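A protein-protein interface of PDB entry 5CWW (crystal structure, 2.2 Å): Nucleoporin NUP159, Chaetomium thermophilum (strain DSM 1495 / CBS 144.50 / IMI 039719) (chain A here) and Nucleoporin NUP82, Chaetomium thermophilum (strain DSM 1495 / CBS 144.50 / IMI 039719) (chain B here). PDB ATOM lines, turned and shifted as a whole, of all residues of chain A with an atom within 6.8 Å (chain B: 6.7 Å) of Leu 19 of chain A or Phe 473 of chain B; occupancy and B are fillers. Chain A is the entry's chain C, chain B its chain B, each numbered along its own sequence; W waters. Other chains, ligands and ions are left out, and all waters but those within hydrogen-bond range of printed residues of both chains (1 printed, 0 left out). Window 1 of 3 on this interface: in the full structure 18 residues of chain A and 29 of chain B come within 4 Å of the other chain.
The side-chain carboxylate of Asp 376 of chain B is in salt-bridge range of the guanidinium group of Arg 16 of chain A (2.5 Å).
O of Asn 25 of chain A lies within hydrogen-bond range of N of Thr 475 of chain B.
The backbone NH of Thr 472 of chain B lies within hydrogen-bond range of the backbone carbonyl oxygen of Asp 376 of chain B (3.0 Å).
The backbone carbonyl oxygen (O) of Ile 439 of chain B is in hydrogen-bond range of the backbone NH (N) of Phe 473 of chain B, 2.8 Å away.
The backbone carbonyl oxygen (O) of Gln 474 of chain B lies within hydrogen-bond range of the backbone NH (N) of Ile 439 of chain B (2.8 Å).
N of Leu 441 of chain B sits at hydrogen-bond distance from O of Leu 471 of chain B.
The side-chain hydroxyl (OG) of Ser 547 of chain B sits at hydrogen-bond distance from the side-chain amide oxygen (OE1) of Gln 474 of chain B, 2.7 Å away.
OE2 of Glu 17 of chain A is in salt-bridge range of NH1 of Arg 16 of chain A (3.5 Å).
Among the printed residues, merely in contact across the chains: Met 14 of chain A with Ile 538 of chain B, Leu 15 of chain A with Leu 441 of chain B, Leu 15 of chain A with Ile 538 of chain B, Arg 16 of chain A with Leu 377 of chain B, Arg 16 of chain A with Leu 471 of chain B, Ser 18 of chain A with Ile 538 of chain B, Ser 18 of chain A with Ala 542 of chain B, Leu 19 of chain A with Leu 377 of chain B, Leu 19 of chain A with Phe 473 of chain B, Leu 19 of chain A with Ala 542 of chain B, Ala 20 of chain A with Leu 377 of chain B, Asn 25 of chain A with Phe 473 of chain B and Asn 25 of chain A with Gln 474 of chain B.
Of the printed residues of chain B, Leu 19 of chain A touches Leu 377 (3.6 Å), Phe 473 (3.98 Å) and Ala 542 (3.9 Å).
Phe 473 of chain B touches two residues of chain A.
Of the printed residues of chain A, Ile 538 of chain B touches Met 14, Leu 15 and Ser 18.
Of the printed residues of chain B, Leu 15 of chain A touches Leu 441 and Ile 538.
Leu 541 of chain B touches none of the printed residues of chain A.
The nearest residue of chain A that does not touch Phe 473 of chain B is Leu 15 of chain A (5.0 Å).
The nearest printed residue of chain B that does not touch Ser 18 of chain A is Lys 543 of chain B (5.3 Å).
Printed residues of chain B that touch a printed residue of chain A: Asp 376, Leu 377, Leu 441, Leu 471, Phe 473, Gln 474, Thr 475, Ile 538 and Ala 542.
Hydrophobic or aromatic side chains of chain B within 4 Å of the printed part of chain A: Leu 377, Leu 441, Leu 471, Phe 473, Ile 538 and Ala 542.
Along chain B the printed residues that touch a printed residue of chain A span positions 376 to 542.
Among the printed residues, 15 pairs touch across the chains.
Among the printed residues, Asp or Glu carboxylates within 4 Å of a Lys or Arg side-chain nitrogen of the other chain: Arg 16 of chain A with Asp 376 of chain B.
Water W1 bridges the side-chain hydroxyl (OG1) of Thr 475 of chain B (3.0 Å) and the backbone carbonyl oxygen (O) of Asn 25 of chain A (3.3 Å).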
ATOM      1  N   MET A  14      -3.081  25.133   0.424  1.00  0.00           N
ATOM      2  CA  MET A  14      -4.085  25.174  -0.632  1.00  0.00           C
ATOM      3  C   MET A  14      -5.124  24.068  -0.469  1.00  0.00           C
ATOM      4  O   MET A  14      -6.290  24.252  -0.816  1.00  0.00           O
ATOM      5  CB  MET A  14      -3.419  25.065  -2.005  1.00  0.00           C
ATOM      6  CG  MET A  14      -2.729  26.345  -2.448  1.00  0.00           C
ATOM      7  SD  MET A  14      -1.796  26.160  -3.980  1.00  0.00           S
ATOM      8  CE  MET A  14      -1.113  27.806  -4.156  1.00  0.00           C
ATOM      9  N   LEU A  15      -4.698  22.923   0.056  1.00  0.00           N
ATOM     10  CA  LEU A  15      -5.619  21.827   0.336  1.00  0.00           C
ATOM     11  C   LEU A  15      -6.636  22.268   1.381  1.00  0.00           C
ATOM     12  O   LEU A  15      -7.839  22.063   1.217  1.00  0.00           O
ATOM     13  CB  LEU A  15      -4.858  20.590   0.818  1.00  0.00           C
ATOM     14  CG  LEU A  15      -5.693  19.409   1.324  1.00  0.00           C
ATOM     15  CD1 LEU A  15      -6.523  18.809   0.203  1.00  0.00           C
ATOM     16  CD2 LEU A  15      -4.795  18.352   1.959  1.00  0.00           C
ATOM     17  N   ARG A  16      -6.133  22.878   2.451  1.00  0.00           N
ATOM     18  CA  ARG A  16      -6.971  23.400   3.526  1.00  0.00           C
ATOM     19  C   ARG A  16      -7.996  24.393   2.979  1.00  0.00           C
ATOM     20  O   ARG A  16      -9.204  24.190   3.125  1.00  0.00           O
ATOM     21  CB  ARG A  16      -6.091  24.046   4.609  1.00  0.00           C
ATOM     22  CG  ARG A  16      -6.747  25.138   5.461  1.00  0.00           C
ATOM     23  CD  ARG A  16      -8.003  24.655   6.161  1.00  0.00           C
ATOM     24  NE  ARG A  16      -8.391  25.526   7.268  1.00  0.00           N
ATOM     25  CZ  ARG A  16      -9.109  26.639   7.149  1.00  0.00           C
ATOM     26  NH1 ARG A  16      -9.531  27.050   5.961  1.00  0.00           N
ATOM     27  NH2 ARG A  16      -9.404  27.346   8.232  1.00  0.00           N
ATOM     28  N   GLU A  17      -7.516  25.454   2.338  1.00  0.00           N
ATOM     29  CA  GLU A  17      -8.403  26.476   1.787  1.00  0.00           C
ATOM     30  C   GLU A  17      -9.374  25.869   0.780  1.00  0.00           C
ATOM     31  O   GLU A  17     -10.529  26.279   0.697  1.00  0.00           O
ATOM     32  CB  GLU A  17      -7.595  27.598   1.127  1.00  0.00           C
ATOM     33  CG  GLU A  17      -6.740  28.404   2.097  1.00  0.00           C
ATOM     34  CD  GLU A  17      -7.548  29.004   3.237  1.00  0.00           C
ATOM     35  OE1 GLU A  17      -8.681  29.467   2.986  1.00  0.00           O
ATOM     36  OE2 GLU A  17      -7.052  29.009   4.383  1.00  0.00           O
ATOM     37  N   SER A  18      -8.905  24.878   0.031  1.00  0.00           N
ATOM     38  CA  SER A  18      -9.751  24.198  -0.939  1.00  0.00           C
ATOM     39  C   SER A  18     -10.846  23.392  -0.243  1.00  0.00           C
ATOM     40  O   SER A  18     -12.004  23.419  -0.655  1.00  0.00           O
ATOM     41  CB  SER A  18      -8.913  23.281  -1.825  1.00  0.00           C
ATOM     42  OG  SER A  18      -9.742  22.524  -2.684  1.00  0.00           O
ATOM     43  N   LEU A  19     -10.471  22.675   0.812  1.00  0.00           N
ATOM     44  CA  LEU A  19     -11.436  21.912   1.600  1.00  0.00           C
ATOM     45  C   LEU A  19     -12.425  22.841   2.298  1.00  0.00           C
ATOM     46  O   LEU A  19     -13.583  22.483   2.510  1.00  0.00           O
ATOM     47  CB  LEU A  19     -10.717  21.038   2.631  1.00  0.00           C
ATOM     48  CG  LEU A  19      -9.959  19.828   2.076  1.00  0.00           C
ATOM     49  CD1 LEU A  19      -9.062  19.225   3.146  1.00  0.00           C
ATOM     50  CD2 LEU A  19     -10.927  18.784   1.540  1.00  0.00           C
ATOM     51  N   ALA A  20     -11.960  24.032   2.660  1.00  0.00           N
ATOM     52  CA  ALA A  20     -12.812  25.023   3.304  1.00  0.00           C
ATOM     53  C   ALA A  20     -13.886  25.550   2.348  1.00  0.00           C
ATOM     54  O   ALA A  20     -15.019  25.796   2.760  1.00  0.00           O
ATOM     55  CB  ALA A  20     -11.972  26.171   3.835  1.00  0.00           C
ATOM     56  N   ARG A  21     -13.528  25.722   1.077  1.00  0.00           N
ATOM     57  CA  ARG A  21     -14.469  26.230   0.081  1.00  0.00           C
ATOM     58  C   ARG A  21     -15.632  25.268  -0.132  1.00  0.00           C
ATOM     59  O   ARG A  21     -16.789  25.682  -0.186  1.00  0.00           O
ATOM     60  CB  ARG A  21     -13.768  26.483  -1.258  1.00  0.00           C
ATOM     61  CG  ARG A  21     -12.903  27.734  -1.294  1.00  0.00           C
ATOM     62  CD  ARG A  21     -12.552  28.122  -2.726  1.00  0.00           C
ATOM     63  NE  ARG A  21     -11.812  27.073  -3.425  1.00  0.00           N
ATOM     64  CZ  ARG A  21     -10.486  26.948  -3.428  1.00  0.00           C
ATOM     65  NH1 ARG A  21      -9.723  27.806  -2.762  1.00  0.00           N
ATOM     66  NH2 ARG A  21      -9.918  25.954  -4.097  1.00  0.00           N
ATOM     67  N   VAL A  22     -15.315  23.983  -0.258  1.00  0.00           N
ATOM     68  CA  VAL A  22     -16.334  22.957  -0.440  1.00  0.00           C
ATOM     69  C   VAL A  22     -17.187  22.837   0.819  1.00  0.00           C
ATOM     70  O   VAL A  22     -18.357  22.457   0.757  1.00  0.00           O
ATOM     71  CB  VAL A  22     -15.702  21.587  -0.773  1.00  0.00           C
ATOM     72  CG1 VAL A  22     -16.776  20.525  -0.989  1.00  0.00           C
ATOM     73  CG2 VAL A  22     -14.818  21.697  -2.007  1.00  0.00           C
ATOM     74  N   GLY A  23     -16.592  23.175   1.959  1.00  0.00           N
ATOM     75  CA  GLY A  23     -17.258  23.048   3.241  1.00  0.00           C
ATOM     76  C   GLY A  23     -16.937  21.705   3.858  1.00  0.00           C
ATOM     77  O   GLY A  23     -16.275  20.881   3.227  1.00  0.00           O
ATOM     78  N   PRO A  24     -17.394  21.476   5.098  1.00  0.00           N
ATOM     79  CA  PRO A  24     -17.151  20.200   5.778  1.00  0.00           C
ATOM     80  C   PRO A  24     -17.619  19.000   4.955  1.00  0.00           C
ATOM     81  O   PRO A  24     -18.818  18.820   4.738  1.00  0.00           O
ATOM     82  CB  PRO A  24     -17.963  20.334   7.072  1.00  0.00           C
ATOM     83  CG  PRO A  24     -18.036  21.798   7.318  1.00  0.00           C
ATOM     84  CD  PRO A  24     -18.109  22.435   5.960  1.00  0.00           C
ATOM     85  N   ASN A  25     -16.666  18.199   4.490  1.00  0.00           N
ATOM     86  CA  ASN A  25     -16.977  16.995   3.734  1.00  0.00           C
ATOM     87  C   ASN A  25     -17.582  15.935   4.649  1.00  0.00           C
ATOM     88  O   ASN A  25     -16.893  15.009   5.081  1.00  0.00           O
ATOM     89  CB  ASN A  25     -15.717  16.460   3.044  1.00  0.00           C
ATOM     90  CG  ASN A  25     -16.004  15.294   2.116  1.00  0.00           C
ATOM     91  OD1 ASN A  25     -17.159  14.996   1.808  1.00  0.00           O
ATOM     92  ND2 ASN A  25     -14.948  14.632   1.654  1.00  0.00           N
ATOM     93  N   ASP B 376      -9.120  21.345  12.686  1.00  0.00           N
ATOM     94  CA  ASP B 376      -9.431  22.394  11.723  1.00  0.00           C
ATOM     95  C   ASP B 376     -10.458  21.875  10.716  1.00  0.00           C
ATOM     96  O   ASP B 376     -10.391  20.720  10.295  1.00  0.00           O
ATOM     97  CB  ASP B 376      -8.156  22.863  11.015  1.00  0.00           C
ATOM     98  CG  ASP B 376      -8.370  24.113  10.185  1.00  0.00           C
ATOM     99  OD1 ASP B 376      -9.370  24.827  10.408  1.00  0.00           O
ATOM    100  OD2 ASP B 376      -7.530  24.382   9.300  1.00  0.00           O
ATOM    101  N   LEU B 377     -11.413  22.730  10.351  1.00  0.00           N
ATOM    102  CA  LEU B 377     -12.527  22.356   9.477  1.00  0.00           C
ATOM    103  C   LEU B 377     -13.333  21.185  10.038  1.00  0.00           C
ATOM    104  O   LEU B 377     -13.889  20.386   9.283  1.00  0.00           O
ATOM    105  CB  LEU B 377     -12.025  22.007   8.074  1.00  0.00           C
ATOM    106  CG  LEU B 377     -11.197  23.063   7.343  1.00  0.00           C
ATOM    107  CD1 LEU B 377     -10.921  22.593   5.926  1.00  0.00           C
ATOM    108  CD2 LEU B 377     -11.897  24.415   7.331  1.00  0.00           C
ATOM    109  N   LYS B 438     -13.535   9.729  11.185  1.00  0.00           N
ATOM    110  CA  LYS B 438     -12.968  11.016  10.818  1.00  0.00           C
ATOM    111  C   LYS B 438     -11.523  10.829  10.376  1.00  0.00           C
ATOM    112  O   LYS B 438     -10.712  10.263  11.108  1.00  0.00           O
ATOM    113  CB  LYS B 438     -13.059  11.991  11.990  1.00  0.00           C
ATOM    114  CG  LYS B 438     -12.791  13.438  11.615  1.00  0.00           C
ATOM    115  CD  LYS B 438     -13.039  14.378  12.788  1.00  0.00           C
ATOM    116  CE  LYS B 438     -14.523  14.499  13.114  1.00  0.00           C
ATOM    117  NZ  LYS B 438     -14.758  15.254  14.371  1.00  0.00           N
ATOM    118  N   ILE B 439     -11.221  11.286   9.166  1.00  0.00           N
ATOM    119  CA  ILE B 439      -9.880  11.175   8.604  1.00  0.00           C
ATOM    120  C   ILE B 439      -9.190  12.529   8.673  1.00  0.00           C
ATOM    121  O   ILE B 439      -9.602  13.479   8.006  1.00  0.00           O
ATOM    122  CB  ILE B 439      -9.909  10.682   7.141  1.00  0.00           C
ATOM    123  CG1 ILE B 439     -10.747   9.405   7.016  1.00  0.00           C
ATOM    124  CG2 ILE B 439      -8.491  10.465   6.619  1.00  0.00           C
ATOM    125  CD1 ILE B 439     -10.258   8.254   7.880  1.00  0.00           C
ATOM    126  N   CYS B 440      -8.147  12.607   9.489  1.00  0.00           N
ATOM    127  CA  CYS B 440      -7.414  13.849   9.694  1.00  0.00           C
ATOM    128  C   CYS B 440      -5.993  13.745   9.164  1.00  0.00           C
ATOM    129  O   CYS B 440      -5.374  12.682   9.228  1.00  0.00           O
ATOM    130  CB  CYS B 440      -7.390  14.211  11.179  1.00  0.00           C
ATOM    131  SG  CYS B 440      -9.024  14.254  11.931  1.00  0.00           S
ATOM    132  N   LEU B 441      -5.481  14.859   8.652  1.00  0.00           N
ATOM    133  CA  LEU B 441      -4.122  14.919   8.133  1.00  0.00           C
ATOM    134  C   LEU B 441      -3.255  15.788   9.030  1.00  0.00           C
ATOM    135  O   LEU B 441      -3.655  16.884   9.430  1.00  0.00           O
ATOM    136  CB  LEU B 441      -4.110  15.463   6.707  1.00  0.00           C
ATOM    137  CG  LEU B 441      -4.922  14.679   5.675  1.00  0.00           C
ATOM    138  CD1 LEU B 441      -4.997  15.455   4.364  1.00  0.00           C
ATOM    139  CD2 LEU B 441      -4.323  13.297   5.452  1.00  0.00           C
ATOM    140  N   LEU B 471      -5.815  18.640  10.387  1.00  0.00           N
ATOM    141  CA  LEU B 471      -6.738  19.043   9.329  1.00  0.00           C
ATOM    142  C   LEU B 471      -7.762  17.947   9.072  1.00  0.00           C
ATOM    143  O   LEU B 471      -7.417  16.866   8.600  1.00  0.00           O
ATOM    144  CB  LEU B 471      -5.978  19.365   8.038  1.00  0.00           C
ATOM    145  CG  LEU B 471      -6.827  19.634   6.787  1.00  0.00           C
ATOM    146  CD1 LEU B 471      -7.781  20.798   7.005  1.00  0.00           C
ATOM    147  CD2 LEU B 471      -5.936  19.895   5.581  1.00  0.00           C
ATOM    148  N   THR B 472      -9.022  18.231   9.382  1.00  0.00           N
ATOM    149  CA  THR B 472     -10.096  17.294   9.092  1.00  0.00           C
ATOM    150  C   THR B 472     -10.305  17.233   7.585  1.00  0.00           C
ATOM    151  O   THR B 472     -10.754  18.202   6.975  1.00  0.00           O
ATOM    152  CB  THR B 472     -11.416  17.693   9.780  1.00  0.00           C
ATOM    153  OG1 THR B 472     -11.179  17.954  11.169  1.00  0.00           O
ATOM    154  CG2 THR B 472     -12.449  16.585   9.646  1.00  0.00           C
ATOM    155  N   PHE B 473      -9.970  16.096   6.989  1.00  0.00           N
ATOM    156  CA  PHE B 473     -10.099  15.929   5.549  1.00  0.00           C
ATOM    157  C   PHE B 473     -11.475  15.398   5.176  1.00  0.00           C
ATOM    158  O   PHE B 473     -12.081  15.850   4.205  1.00  0.00           O
ATOM    159  CB  PHE B 473      -9.024  14.986   5.011  1.00  0.00           C
ATOM    160  CG  PHE B 473      -9.327  14.468   3.638  1.00  0.00           C
ATOM    161  CD1 PHE B 473      -9.242  15.301   2.535  1.00  0.00           C
ATOM    162  CD2 PHE B 473      -9.716  13.152   3.452  1.00  0.00           C
ATOM    163  CE1 PHE B 473      -9.535  14.830   1.270  1.00  0.00           C
ATOM    164  CE2 PHE B 473     -10.007  12.674   2.188  1.00  0.00           C
ATOM    165  CZ  PHE B 473      -9.920  13.514   1.097  1.00  0.00           C
ATOM    166  N   GLN B 474     -11.966  14.445   5.958  1.00  0.00           N
ATOM    167  CA  GLN B 474     -13.228  13.791   5.651  1.00  0.00           C
ATOM    168  C   GLN B 474     -13.861  13.178   6.899  1.00  0.00           C
ATOM    169  O   GLN B 474     -13.165  12.725   7.808  1.00  0.00           O
ATOM    170  CB  GLN B 474     -13.008  12.721   4.579  1.00  0.00           C
ATOM    171  CG  GLN B 474     -14.261  11.989   4.154  1.00  0.00           C
ATOM    172  CD  GLN B 474     -13.997  11.003   3.032  1.00  0.00           C
ATOM    173  OE1 GLN B 474     -12.852  10.631   2.773  1.00  0.00           O
ATOM    174  NE2 GLN B 474     -15.059  10.580   2.355  1.00  0.00           N
ATOM    175  N   THR B 475     -15.190  13.175   6.924  1.00  0.00           N
ATOM    176  CA  THR B 475     -15.953  12.579   8.011  1.00  0.00           C
ATOM    177  C   THR B 475     -17.142  11.838   7.419  1.00  0.00           C
ATOM    178  O   THR B 475     -17.879  12.402   6.614  1.00  0.00           O
ATOM    179  CB  THR B 475     -16.459  13.641   9.011  1.00  0.00           C
ATOM    180  OG1 THR B 475     -15.370  14.472   9.430  1.00  0.00           O
ATOM    181  CG2 THR B 475     -17.096  12.983  10.230  1.00  0.00           C
ATOM    182  N   LEU B 515      -8.048   4.502   1.749  1.00  0.00           N
ATOM    183  CA  LEU B 515      -7.678   5.878   1.435  1.00  0.00           C
ATOM    184  C   LEU B 515      -6.893   5.972   0.130  1.00  0.00           C
ATOM    185  O   LEU B 515      -6.493   7.061  -0.278  1.00  0.00           O
ATOM    186  CB  LEU B 515      -6.858   6.475   2.579  1.00  0.00           C
ATOM    187  CG  LEU B 515      -7.455   6.264   3.971  1.00  0.00           C
ATOM    188  CD1 LEU B 515      -6.607   6.954   5.031  1.00  0.00           C
ATOM    189  CD2 LEU B 515      -8.894   6.751   4.029  1.00  0.00           C
ATOM    190  N   TRP B 518      -6.384   7.936  -3.330  1.00  0.00           N
ATOM    191  CA  TRP B 518      -6.411   9.359  -3.004  1.00  0.00           C
ATOM    192  C   TRP B 518      -5.142   9.842  -2.304  1.00  0.00           C
ATOM    193  O   TRP B 518      -4.676  10.951  -2.568  1.00  0.00           O
ATOM    194  CB  TRP B 518      -7.621   9.683  -2.128  1.00  0.00           C
ATOM    195  CG  TRP B 518      -7.522  11.039  -1.517  1.00  0.00           C
ATOM    196  CD1 TRP B 518      -7.869  12.226  -2.088  1.00  0.00           C
ATOM    197  CD2 TRP B 518      -7.023  11.350  -0.210  1.00  0.00           C
ATOM    198  NE1 TRP B 518      -7.619  13.259  -1.216  1.00  0.00           N
ATOM    199  CE2 TRP B 518      -7.097  12.747  -0.058  1.00  0.00           C
ATOM    200  CE3 TRP B 518      -6.520  10.582   0.843  1.00  0.00           C
ATOM    201  CZ2 TRP B 518      -6.691  13.392   1.109  1.00  0.00           C
ATOM    202  CZ3 TRP B 518      -6.120  11.224   2.000  1.00  0.00           C
ATOM    203  CH2 TRP B 518      -6.207  12.614   2.124  1.00  0.00           C
ATOM    204  N   ILE B 538      -4.946  20.826  -6.829  1.00  0.00           N
ATOM    205  CA  ILE B 538      -5.380  20.536  -5.462  1.00  0.00           C
ATOM    206  C   ILE B 538      -6.897  20.652  -5.344  1.00  0.00           C
ATOM    207  O   ILE B 538      -7.529  19.900  -4.601  1.00  0.00           O
ATOM    208  CB  ILE B 538      -4.705  21.477  -4.432  1.00  0.00           C
ATOM    209  CG1 ILE B 538      -3.214  21.146  -4.297  1.00  0.00           C
ATOM    210  CG2 ILE B 538      -5.371  21.369  -3.059  1.00  0.00           C
ATOM    211  CD1 ILE B 538      -2.913  19.780  -3.682  1.00  0.00           C
ATOM    212  N   LEU B 541      -8.495  17.514  -6.418  1.00  0.00           N
ATOM    213  CA  LEU B 541      -8.257  16.470  -5.431  1.00  0.00           C
ATOM    214  C   LEU B 541      -9.190  16.612  -4.231  1.00  0.00           C
ATOM    215  O   LEU B 541      -9.716  15.621  -3.726  1.00  0.00           O
ATOM    216  CB  LEU B 541      -6.796  16.506  -4.977  1.00  0.00           C
ATOM    217  CG  LEU B 541      -6.343  15.406  -4.019  1.00  0.00           C
ATOM    218  CD1 LEU B 541      -4.917  14.988  -4.330  1.00  0.00           C
ATOM    219  CD2 LEU B 541      -6.440  15.886  -2.579  1.00  0.00           C
ATOM    220  N   ALA B 542      -9.397  17.846  -3.781  1.00  0.00           N
ATOM    221  CA  ALA B 542     -10.312  18.113  -2.676  1.00  0.00           C
ATOM    222  C   ALA B 542     -11.753  17.844  -3.093  1.00  0.00           C
ATOM    223  O   ALA B 542     -12.598  17.510  -2.261  1.00  0.00           O
ATOM    224  CB  ALA B 542     -10.161  19.543  -2.197  1.00  0.00           C
ATOM    225  N   LYS B 543     -12.026  17.999  -4.385  1.00  0.00           N
ATOM    226  CA  LYS B 543     -13.347  17.714  -4.936  1.00  0.00           C
ATOM    227  C   LYS B 543     -13.524  16.217  -5.176  1.00  0.00           C
ATOM    228  O   LYS B 543     -14.647  15.727  -5.288  1.00  0.00           O
ATOM    229  CB  LYS B 543     -13.552  18.488  -6.240  1.00  0.00           C
ATOM    230  CG  LYS B 543     -13.865  19.962  -6.034  1.00  0.00           C
ATOM    231  CD  LYS B 543     -14.017  20.690  -7.357  1.00  0.00           C
ATOM    232  CE  LYS B 543     -14.391  22.147  -7.146  1.00  0.00           C
ATOM    233  NZ  LYS B 543     -14.573  22.874  -8.433  1.00  0.00           N
ATOM    234  N   GLY B 544     -12.409  15.497  -5.252  1.00  0.00           N
ATOM    235  CA  GLY B 544     -12.433  14.048  -5.359  1.00  0.00           C
ATOM    236  C   GLY B 544     -13.092  13.425  -4.144  1.00  0.00           C
ATOM    237  O   GLY B 544     -12.991  13.958  -3.040  1.00  0.00           O
ATOM    238  N   GLN B 545     -13.772  12.300  -4.342  1.00  0.00           N
ATOM    239  CA  GLN B 545     -14.513  11.664  -3.257  1.00  0.00           C
ATOM    240  C   GLN B 545     -13.576  11.072  -2.207  1.00  0.00           C
ATOM    241  O   GLN B 545     -14.007  10.719  -1.108  1.00  0.00           O
ATOM    242  CB  GLN B 545     -15.430  10.569  -3.807  1.00  0.00           C
ATOM    243  CG  GLN B 545     -16.417  11.057  -4.854  1.00  0.00           C
ATOM    244  CD  GLN B 545     -17.450  10.007  -5.214  1.00  0.00           C
ATOM    245  OE1 GLN B 545     -17.587   9.627  -6.376  1.00  0.00           O
ATOM    246  NE2 GLN B 545     -18.184   9.532  -4.214  1.00  0.00           N
ATOM    247  N   GLY B 546     -12.297  10.965  -2.549  1.00  0.00           N
ATOM    248  CA  GLY B 546     -11.296  10.501  -1.606  1.00  0.00           C
ATOM    249  C   GLY B 546     -11.445   9.034  -1.259  1.00  0.00           C
ATOM    250  O   GLY B 546     -11.403   8.167  -2.131  1.00  0.00           O
ATOM    251  N   SER B 547     -11.621   8.760   0.030  1.00  0.00           N
ATOM    252  CA  SER B 547     -11.663   7.390   0.528  1.00  0.00           C
ATOM    253  C   SER B 547     -12.911   6.648   0.066  1.00  0.00           C
ATOM    254  O   SER B 547     -13.963   7.253  -0.142  1.00  0.00           O
ATOM    255  CB  SER B 547     -11.603   7.382   2.057  1.00  0.00           C
ATOM    256  OG  SER B 547     -12.800   7.897   2.613  1.00  0.00           O
HETATM  257  O   HOH W   1     -15.286  16.694   7.444  1.00  0.00           O
